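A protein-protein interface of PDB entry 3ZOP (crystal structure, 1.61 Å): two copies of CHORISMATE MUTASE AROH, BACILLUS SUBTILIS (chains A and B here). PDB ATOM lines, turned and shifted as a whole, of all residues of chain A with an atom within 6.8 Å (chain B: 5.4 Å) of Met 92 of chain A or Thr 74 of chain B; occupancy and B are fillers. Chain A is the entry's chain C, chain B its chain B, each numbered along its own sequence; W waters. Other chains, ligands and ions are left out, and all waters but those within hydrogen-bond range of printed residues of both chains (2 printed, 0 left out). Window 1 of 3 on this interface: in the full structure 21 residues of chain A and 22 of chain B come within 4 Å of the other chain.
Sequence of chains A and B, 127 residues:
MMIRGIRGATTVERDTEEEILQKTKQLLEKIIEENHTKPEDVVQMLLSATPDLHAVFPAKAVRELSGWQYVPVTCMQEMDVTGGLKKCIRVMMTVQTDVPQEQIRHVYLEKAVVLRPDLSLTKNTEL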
ATOM      1  N   ARG A   4      -7.368  14.486  -6.614  1.00  0.00           N
ATOM      2  CA  ARG A   4      -7.070  13.148  -7.110  1.00  0.00           C
ATOM      3  C   ARG A   4      -8.272  12.524  -7.788  1.00  0.00           C
ATOM      4  O   ARG A   4      -9.410  12.733  -7.368  1.00  0.00           O
ATOM      5  CB  ARG A   4      -6.577  12.247  -5.965  1.00  0.00           C
ATOM      6  CG  ARG A   4      -5.283  12.766  -5.360  1.00  0.00           C
ATOM      7  CD  ARG A   4      -4.287  11.709  -4.979  1.00  0.00           C
ATOM      8  NE  ARG A   4      -3.069  12.344  -4.495  1.00  0.00           N
ATOM      9  CZ  ARG A   4      -1.984  12.547  -5.239  1.00  0.00           C
ATOM     10  NH1 ARG A   4      -1.944  12.126  -6.501  1.00  0.00           N
ATOM     11  NH2 ARG A   4      -0.929  13.144  -4.705  1.00  0.00           N
ATOM     12  N   GLY A   5      -8.022  11.741  -8.834  1.00  0.00           N
ATOM     13  CA  GLY A   5      -9.111  11.027  -9.496  1.00  0.00           C
ATOM     14  C   GLY A   5      -9.404   9.732  -8.752  1.00  0.00           C
ATOM     15  O   GLY A   5      -8.475   9.049  -8.301  1.00  0.00           O
ATOM     16  N   ILE A   6     -10.691   9.392  -8.635  1.00  0.00           N
ATOM     17  CA  ILE A   6     -11.117   8.094  -8.109  1.00  0.00           C
ATOM     18  C   ILE A   6     -11.859   7.366  -9.228  1.00  0.00           C
ATOM     19  O   ILE A   6     -12.815   7.901  -9.791  1.00  0.00           O
ATOM     20  CB  ILE A   6     -12.029   8.226  -6.875  1.00  0.00           C
ATOM     21  CG1 ILE A   6     -11.410   9.181  -5.844  1.00  0.00           C
ATOM     22  CG2 ILE A   6     -12.283   6.824  -6.278  1.00  0.00           C
ATOM     23  CD1 ILE A   6     -12.217   9.307  -4.546  1.00  0.00           C
ATOM     24  N   ARG A   7     -11.403   6.166  -9.568  1.00  0.00           N
ATOM     25  CA  ARG A   7     -12.040   5.391 -10.633  1.00  0.00           C
ATOM     26  C   ARG A   7     -13.029   4.385 -10.075  1.00  0.00           C
ATOM     27  O   ARG A   7     -12.811   3.808  -8.998  1.00  0.00           O
ATOM     28  CB  ARG A   7     -10.999   4.641 -11.473  1.00  0.00           C
ATOM     29  CG  ARG A   7     -10.267   5.482 -12.504  1.00  0.00           C
ATOM     30  CD  ARG A   7     -11.175   5.818 -13.690  1.00  0.00           C
ATOM     31  NE  ARG A   7     -12.184   4.788 -13.935  1.00  0.00           N
ATOM     32  CZ  ARG A   7     -11.956   3.618 -14.529  1.00  0.00           C
ATOM     33  NH1 ARG A   7     -10.741   3.300 -14.955  1.00  0.00           N
ATOM     34  NH2 ARG A   7     -12.955   2.761 -14.708  1.00  0.00           N
ATOM     35  N   GLY A   8     -14.101   4.174 -10.838  1.00  0.00           N
ATOM     36  CA  GLY A   8     -15.069   3.118 -10.591  1.00  0.00           C
ATOM     37  C   GLY A   8     -15.430   2.476 -11.923  1.00  0.00           C
ATOM     38  O   GLY A   8     -15.340   3.108 -12.977  1.00  0.00           O
ATOM     39  N   ILE A  31     -18.033   3.894  -3.903  1.00  0.00           N
ATOM     40  CA  ILE A  31     -16.936   4.855  -3.941  1.00  0.00           C
ATOM     41  C   ILE A  31     -16.987   5.826  -2.767  1.00  0.00           C
ATOM     42  O   ILE A  31     -15.965   6.074  -2.117  1.00  0.00           O
ATOM     43  CB  ILE A  31     -16.936   5.639  -5.255  1.00  0.00           C
ATOM     44  CG1 ILE A  31     -16.631   4.686  -6.414  1.00  0.00           C
ATOM     45  CG2 ILE A  31     -15.940   6.826  -5.185  1.00  0.00           C
ATOM     46  CD1 ILE A  31     -16.730   5.308  -7.808  1.00  0.00           C
ATOM     47  N   GLN A  44     -15.481  17.586 -10.083  1.00  0.00           N
ATOM     48  CA  GLN A  44     -16.341  17.227 -11.202  1.00  0.00           C
ATOM     49  C   GLN A  44     -16.317  15.720 -11.340  1.00  0.00           C
ATOM     50  O   GLN A  44     -15.465  15.054 -10.751  1.00  0.00           O
ATOM     51  CB  GLN A  44     -15.855  17.853 -12.517  1.00  0.00           C
ATOM     52  CG  GLN A  44     -14.484  17.362 -12.987  1.00  0.00           C
ATOM     53  CD  GLN A  44     -13.865  18.315 -13.992  1.00  0.00           C
ATOM     54  OE1 GLN A  44     -13.877  19.533 -13.773  1.00  0.00           O
ATOM     55  NE2 GLN A  44     -13.323  17.776 -15.109  1.00  0.00           N
ATOM     56  N   MET A  45     -17.235  15.176 -12.127  1.00  0.00           N
ATOM     57  CA  MET A  45     -17.205  13.733 -12.401  1.00  0.00           C
ATOM     58  C   MET A  45     -17.412  13.473 -13.872  1.00  0.00           C
ATOM     59  O   MET A  45     -18.164  14.188 -14.529  1.00  0.00           O
ATOM     60  CB  MET A  45     -18.308  13.018 -11.644  1.00  0.00           C
ATOM     61  CG  MET A  45     -18.200  13.108 -10.168  1.00  0.00           C
ATOM     62  SD  MET A  45     -19.480  12.112  -9.387  1.00  0.00           S
ATOM     63  CE  MET A  45     -19.449  10.672 -10.421  1.00  0.00           C
ATOM     64  N   LEU A  46     -16.750  12.434 -14.367  1.00  0.00           N
ATOM     65  CA  LEU A  46     -16.904  11.992 -15.746  1.00  0.00           C
ATOM     66  C   LEU A  46     -17.439  10.573 -15.709  1.00  0.00           C
ATOM     67  O   LEU A  46     -16.844   9.709 -15.076  1.00  0.00           O
ATOM     68  CB  LEU A  46     -15.546  12.034 -16.467  1.00  0.00           C
ATOM     69  CG  LEU A  46     -15.433  11.908 -17.987  1.00  0.00           C
ATOM     70  CD1 LEU A  46     -16.198  13.018 -18.692  1.00  0.00           C
ATOM     71  CD2 LEU A  46     -13.965  11.987 -18.361  1.00  0.00           C
ATOM     72  N   LEU A  47     -18.573  10.337 -16.351  1.00  0.00           N
ATOM     73  CA  LEU A  47     -19.077   8.976 -16.471  1.00  0.00           C
ATOM     74  C   LEU A  47     -18.993   8.564 -17.940  1.00  0.00           C
ATOM     75  O   LEU A  47     -19.111   9.407 -18.840  1.00  0.00           O
ATOM     76  CB  LEU A  47     -20.532   8.914 -15.990  1.00  0.00           C
ATOM     77  CG  LEU A  47     -20.742   9.032 -14.486  1.00  0.00           C
ATOM     78  CD1 LEU A  47     -22.119   9.610 -14.212  1.00  0.00           C
ATOM     79  CD2 LEU A  47     -20.659   7.662 -13.893  1.00  0.00           C
ATOM     80  N   SER A  48     -18.746   7.283 -18.189  1.00  0.00           N
ATOM     81  CA  SER A  48     -18.736   6.781 -19.551  1.00  0.00           C
ATOM     82  C   SER A  48     -19.502   5.480 -19.659  1.00  0.00           C
ATOM     83  O   SER A  48     -19.724   4.783 -18.668  1.00  0.00           O
ATOM     84  CB  SER A  48     -17.308   6.552 -20.035  1.00  0.00           C
ATOM     85  OG  SER A  48     -16.713   5.487 -19.315  1.00  0.00           O
ATOM     86  N   GLU A  78     -17.255   5.496 -23.940  1.00  0.00           N
ATOM     87  CA  GLU A  78     -16.034   4.743 -23.797  1.00  0.00           C
ATOM     88  C   GLU A  78     -15.523   4.290 -25.158  1.00  0.00           C
ATOM     89  O   GLU A  78     -16.289   4.040 -26.082  1.00  0.00           O
ATOM     90  CB  GLU A  78     -16.304   3.526 -22.913  1.00  0.00           C
ATOM     91  CG  GLU A  78     -15.144   2.570 -22.901  1.00  0.00           C
ATOM     92  CD  GLU A  78     -14.764   2.148 -21.523  1.00  0.00           C
ATOM     93  OE1 GLU A  78     -15.610   1.505 -20.829  1.00  0.00           O
ATOM     94  OE2 GLU A  78     -13.610   2.472 -21.143  1.00  0.00           O
ATOM     95  C   CIR A  90     -17.301   5.124 -15.063  1.00  0.00           C
ATOM     96  O   CIR A  90     -18.029   5.963 -15.650  1.00  0.00           O
ATOM     97  CA  CIR A  90     -17.069   3.765 -15.665  1.00  0.00           C
ATOM     98  N   CIR A  90     -18.234   3.371 -16.442  1.00  0.00           N
ATOM     99  C3  CIR A  90     -15.830   3.765 -16.568  1.00  0.00           C
ATOM    100  C4  CIR A  90     -15.498   2.334 -16.990  1.00  0.00           C
ATOM    101  C5  CIR A  90     -14.310   2.193 -17.939  1.00  0.00           C
ATOM    102  N6  CIR A  90     -14.248   0.791 -18.347  1.00  0.00           N
ATOM    103  C7  CIR A  90     -13.238   0.106 -18.895  1.00  0.00           C
ATOM    104  O7  CIR A  90     -12.062   0.324 -18.620  1.00  0.00           O
ATOM    105  N8  CIR A  90     -13.564  -0.876 -19.752  1.00  0.00           N
ATOM    106  N   VAL A  91     -16.612   5.448 -14.053  1.00  0.00           N
ATOM    107  CA  VAL A  91     -16.611   6.738 -13.333  1.00  0.00           C
ATOM    108  C   VAL A  91     -15.189   7.200 -13.138  1.00  0.00           C
ATOM    109  O   VAL A  91     -14.309   6.401 -12.783  1.00  0.00           O
ATOM    110  CB  VAL A  91     -17.200   6.581 -11.920  1.00  0.00           C
ATOM    111  CG1 VAL A  91     -17.016   7.875 -11.128  1.00  0.00           C
ATOM    112  CG2 VAL A  91     -18.676   6.174 -12.012  1.00  0.00           C
ATOM    113  N   MET A  92     -14.972   8.487 -13.372  1.00  0.00           N
ATOM    114  CA  MET A  92     -13.786   9.201 -12.880  1.00  0.00           C
ATOM    115  C   MET A  92     -14.264  10.378 -12.043  1.00  0.00           C
ATOM    116  O   MET A  92     -14.762  11.386 -12.562  1.00  0.00           O
ATOM    117  CB  MET A  92     -12.878   9.714 -14.010  1.00  0.00           C
ATOM    118  CG  MET A  92     -11.600  10.426 -13.488  1.00  0.00           C
ATOM    119  SD  MET A  92     -10.408   9.265 -12.750  1.00  0.00           S
ATOM    120  CE  MET A  92      -9.733   8.578 -14.247  1.00  0.00           C
ATOM    121  N   MET A  93     -14.121  10.243 -10.737  1.00  0.00           N
ATOM    122  CA  MET A  93     -14.611  11.243  -9.807  1.00  0.00           C
ATOM    123  C   MET A  93     -13.398  12.014  -9.303  1.00  0.00           C
ATOM    124  O   MET A  93     -12.542  11.431  -8.637  1.00  0.00           O
ATOM    125  CB  MET A  93     -15.307  10.526  -8.636  1.00  0.00           C
ATOM    126  CG  MET A  93     -16.016  11.451  -7.663  1.00  0.00           C
ATOM    127  SD  MET A  93     -16.550  10.629  -6.114  1.00  0.00           S
ATOM    128  CE  MET A  93     -17.952   9.618  -6.623  1.00  0.00           C
ATOM    129  N   THR A  94     -13.316  13.309  -9.617  1.00  0.00           N
ATOM    130  CA  THR A  94     -12.157  14.117  -9.239  1.00  0.00           C
ATOM    131  C   THR A  94     -12.461  14.821  -7.935  1.00  0.00           C
ATOM    132  O   THR A  94     -13.441  15.557  -7.853  1.00  0.00           O
ATOM    133  CB  THR A  94     -11.849  15.166 -10.321  1.00  0.00           C
ATOM    134  OG1 THR A  94     -11.746  14.493 -11.577  1.00  0.00           O
ATOM    135  CG2 THR A  94     -10.538  15.869 -10.021  1.00  0.00           C
ATOM    136  N   HIS A 106     -10.154   2.753  -5.421  1.00  0.00           N
ATOM    137  CA  HIS A 106     -10.896   2.607  -6.670  1.00  0.00           C
ATOM    138  C   HIS A 106     -11.793   1.380  -6.563  1.00  0.00           C
ATOM    139  O   HIS A 106     -11.461   0.415  -5.856  1.00  0.00           O
ATOM    140  CB  HIS A 106      -9.934   2.505  -7.851  1.00  0.00           C
ATOM    141  CG  HIS A 106      -8.914   3.602  -7.875  1.00  0.00           C
ATOM    142  ND1 HIS A 106      -9.216   4.890  -8.270  1.00  0.00           N
ATOM    143  CD2 HIS A 106      -7.610   3.613  -7.514  1.00  0.00           C
ATOM    144  CE1 HIS A 106      -8.130   5.639  -8.177  1.00  0.00           C
ATOM    145  NE2 HIS A 106      -7.143   4.888  -7.716  1.00  0.00           N
ATOM    146  N   GLN B  44      -4.997  12.753 -12.505  1.00  0.00           N
ATOM    147  CA  GLN B  44      -5.659  11.745 -13.337  1.00  0.00           C
ATOM    148  C   GLN B  44      -5.229  11.974 -14.774  1.00  0.00           C
ATOM    149  O   GLN B  44      -4.660  13.028 -15.099  1.00  0.00           O
ATOM    150  CB  GLN B  44      -7.181  11.870 -13.238  1.00  0.00           C
ATOM    151  CG  GLN B  44      -7.740  13.184 -13.808  1.00  0.00           C
ATOM    152  CD  GLN B  44      -9.171  13.436 -13.364  1.00  0.00           C
ATOM    153  OE1 GLN B  44      -9.492  13.300 -12.180  1.00  0.00           O
ATOM    154  NE2 GLN B  44     -10.046  13.789 -14.310  1.00  0.00           N
ATOM    155  N   MET B  45      -5.493  10.995 -15.631  1.00  0.00           N
ATOM    156  CA  MET B  45      -5.264  11.176 -17.051  1.00  0.00           C
ATOM    157  C   MET B  45      -6.481  10.722 -17.832  1.00  0.00           C
ATOM    158  O   MET B  45      -7.154   9.769 -17.441  1.00  0.00           O
ATOM    159  CB  MET B  45      -4.052  10.361 -17.521  1.00  0.00           C
ATOM    160  CG  MET B  45      -2.802  10.641 -16.773  1.00  0.00           C
ATOM    161  SD  MET B  45      -1.373   9.920 -17.601  1.00  0.00           S
ATOM    162  CE  MET B  45      -1.995   9.672 -19.250  1.00  0.00           C
ATOM    163  N   LEU B  46      -6.737  11.408 -18.938  1.00  0.00           N
ATOM    164  CA  LEU B  46      -7.784  11.015 -19.877  1.00  0.00           C
ATOM    165  C   LEU B  46      -7.123  10.719 -21.220  1.00  0.00           C
ATOM    166  O   LEU B  46      -6.398  11.546 -21.765  1.00  0.00           O
ATOM    167  CB  LEU B  46      -8.832  12.124 -20.012  1.00  0.00           C
ATOM    168  CG  LEU B  46     -10.103  11.892 -20.848  1.00  0.00           C
ATOM    169  CD1 LEU B  46     -10.891  10.660 -20.409  1.00  0.00           C
ATOM    170  CD2 LEU B  46     -10.979  13.150 -20.758  1.00  0.00           C
ATOM    171  N   LEU B  47      -7.369   9.529 -21.747  1.00  0.00           N
ATOM    172  CA  LEU B  47      -6.841   9.167 -23.052  1.00  0.00           C
ATOM    173  C   LEU B  47      -8.026   9.067 -23.994  1.00  0.00           C
ATOM    174  O   LEU B  47      -9.114   8.646 -23.593  1.00  0.00           O
ATOM    175  CB  LEU B  47      -6.134   7.817 -22.995  1.00  0.00           C
ATOM    176  CG  LEU B  47      -4.887   7.791 -22.113  1.00  0.00           C
ATOM    177  CD1 LEU B  47      -4.417   6.349 -21.939  1.00  0.00           C
ATOM    178  CD2 LEU B  47      -3.828   8.618 -22.769  1.00  0.00           C
ATOM    179  N   PRO B  72      -4.731   7.253 -11.888  1.00  0.00           N
ATOM    180  CA  PRO B  72      -6.019   6.849 -12.461  1.00  0.00           C
ATOM    181  C   PRO B  72      -6.191   7.346 -13.886  1.00  0.00           C
ATOM    182  O   PRO B  72      -5.879   8.500 -14.191  1.00  0.00           O
ATOM    183  CB  PRO B  72      -7.048   7.513 -11.540  1.00  0.00           C
ATOM    184  CG  PRO B  72      -6.349   8.680 -10.958  1.00  0.00           C
ATOM    185  CD  PRO B  72      -4.873   8.339 -10.898  1.00  0.00           C
ATOM    186  N   VAL B  73      -6.689   6.483 -14.757  1.00  0.00           N
ATOM    187  CA  VAL B  73      -6.795   6.828 -16.151  1.00  0.00           C
ATOM    188  C   VAL B  73      -8.095   6.266 -16.697  1.00  0.00           C
ATOM    189  O   VAL B  73      -8.560   5.212 -16.263  1.00  0.00           O
ATOM    190  CB  VAL B  73      -5.584   6.253 -16.922  1.00  0.00           C
ATOM    191  CG1 VAL B  73      -5.378   4.793 -16.573  1.00  0.00           C
ATOM    192  CG2 VAL B  73      -5.732   6.486 -18.433  1.00  0.00           C
ATOM    193  N   THR B  74      -8.706   6.977 -17.628  1.00  0.00           N
ATOM    194  CA  THR B  74      -9.807   6.377 -18.342  1.00  0.00           C
ATOM    195  C   THR B  74      -9.718   6.722 -19.821  1.00  0.00           C
ATOM    196  O   THR B  74      -9.014   7.660 -20.184  1.00  0.00           O
ATOM    197  CB  THR B  74     -11.141   6.713 -17.729  1.00  0.00           C
ATOM    198  OG1 THR B  74     -12.038   5.621 -17.979  1.00  0.00           O
ATOM    199  CG2 THR B  74     -11.651   8.008 -18.316  1.00  0.00           C
ATOM    200  N   CYS B  75     -10.378   5.939 -20.658  1.00  0.00           N
ATOM    201  CA  CYS B  75     -10.288   6.155 -22.079  1.00  0.00           C
ATOM    202  C   CYS B  75     -11.640   6.630 -22.582  1.00  0.00           C
ATOM    203  O   CYS B  75     -12.665   6.430 -21.918  1.00  0.00           O
ATOM    204  CB  CYS B  75      -9.842   4.867 -22.770  1.00  0.00           C
ATOM    205  SG  CYS B  75      -8.362   4.158 -22.002  1.00  0.00           S
ATOM    206  N   MET B  76     -11.637   7.288 -23.732  1.00  0.00           N
ATOM    207  CA  MET B  76     -12.860   7.772 -24.316  1.00  0.00           C
ATOM    208  C   MET B  76     -12.717   7.800 -25.820  1.00  0.00           C
ATOM    209  O   MET B  76     -11.606   7.730 -26.351  1.00  0.00           O
ATOM    210  CB  MET B  76     -13.154   9.181 -23.820  1.00  0.00           C
ATOM    211  CG  MET B  76     -14.543   9.339 -23.278  1.00  0.00           C
ATOM    212  SD  MET B  76     -14.754   8.322 -21.811  1.00  0.00           S
ATOM    213  CE  MET B  76     -13.528   9.047 -20.727  1.00  0.00           C
HETATM  214  O   HOH W   1     -14.060   5.788 -19.770  1.00  0.00           O
HETATM  215  O   HOH W   2     -11.459   3.360 -19.777  1.00  0.00           O
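The backbone NH (N) of Met 45 of chain B sits at hydrogen-bond distance from the backbone carbonyl oxygen (O) of Pro 72 of chain B (2.9 Å).
The backbone carbonyl oxygen of Met 45 of chain B sits at hydrogen-bond distance from the backbone NH of Thr 74 of chain B.
The backbone NH (N) of Leu 47 of chain B is in hydrogen-bond range of the backbone carbonyl oxygen (O) of Thr 74 of chain B, at 2.9 Å.
O of Leu 47 of chain B sits at hydrogen-bond distance from N of Met 76 of chain B, 2.9 Å away.
N of Thr 94 of chain A lies within hydrogen-bond range of O of Gln 44 of chain A (3.0 Å).
The backbone NH (N) of Ser 48 of chain A is in hydrogen-bond range of O of CIR 90 of chain A (3.0 Å).
Leu 46 of chain A touches its own counterpart, Leu 46 of chain B.
Of the 14 pairs that touch across the chains among the printed residues, 1 has its exchanged pair printed and touching as well.
Met 92 of chain A touches just these residues of chain B: Gln 44, Pro 72, Val 73 and Thr 74.
Of the printed residues of chain A, Thr 74 of chain B touches Arg 7 and Met 92.
Printed residues of chain B within 4 Å of Ser 48 of chain A: Met 76 (3.6 Å).
Of the printed residues of chain B, Leu 46 of chain A touches Leu 46 (3.9 Å) and Met 76 (3.8 Å).
Of the printed residues of chain B, His 106 of chain A touches Pro 72.
The nearest printed residue of chain B that does not touch Thr 94 of chain A is Pro 72 of chain B (8.0 Å).
Water W1 lies within hydrogen-bond range of the backbone carbonyl oxygen (O) of Cys 75 of chain B, the side-chain hydroxyl (OG1) of Thr 74 of chain B, the side-chain hydroxyl (OG) of Ser 48 of chain A and the side-chain sulfur (SD) of Met 76 of chain B.
Water W2 lies within hydrogen-bond range of OE2 of Glu 78 of chain A, N of Cys 75 of chain B, OG1 of Thr 74 of chain B and O7 of CIR 90 of chain A.
Among the printed residues, merely in contact across the chains: Gly 5 of chain A with Pro 72 of chain B (3.4 Å), Gly 5 of chain A with Gln 44 of chain B (3.5 Å), Ser 48 of chain A with Met 76 of chain B (3.6 Å), Met 92 of chain A with Val 73 of chain B (3.7 Å), Met 92 of chain A with Pro 72 of chain B (3.8 Å), Met 92 of chain A with Gln 44 of chain B (3.8 Å), Leu 46 of chain A with Met 76 of chain B (3.8 Å), Met 92 of chain A with Thr 74 of chain B (3.9 Å), Leu 46 of chain A with Leu 46 of chain B (3.9 Å), Arg 7 of chain A with Pro 72 of chain B (3.9 Å), Arg 7 of chain A with Thr 74 of chain B (3.99 Å) and His 106 of chain A with Pro 72 of chain B (3.999 Å).
Printed residues of chain A that touch a printed residue of chain B: Gly 5, Arg 7, Leu 46, Ser 48, Met 92, Thr 94 and His 106.
Hydrophobic or aromatic side chains of chain A that line the printed part of chain B: Leu 46, Met 92 and His 106.
Of the 9 printed residues of chain B, 6 touch a printed residue of chain A.
Hydrophobic or aromatic side chains of chain B that line the printed part of chain A: Leu 46, Pro 72 and Met 76.
Along chain B the printed residues that touch a printed residue of chain A span positions 44 to 76.
Among the printed residues, 14 pairs touch across the chains.
Among the printed residues, no Asp or Glu carboxylate lies within 4 Å of a Lys or Arg side-chain nitrogen of the other chain.
OE1 of Gln 44 of chain B lies within hydrogen-bond range of OG1 of Thr 94 of chain A (2.6 Å).
O of Val 73 of chain B lies within hydrogen-bond range of NH1 of Arg 7 of chain A (3.2 Å).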
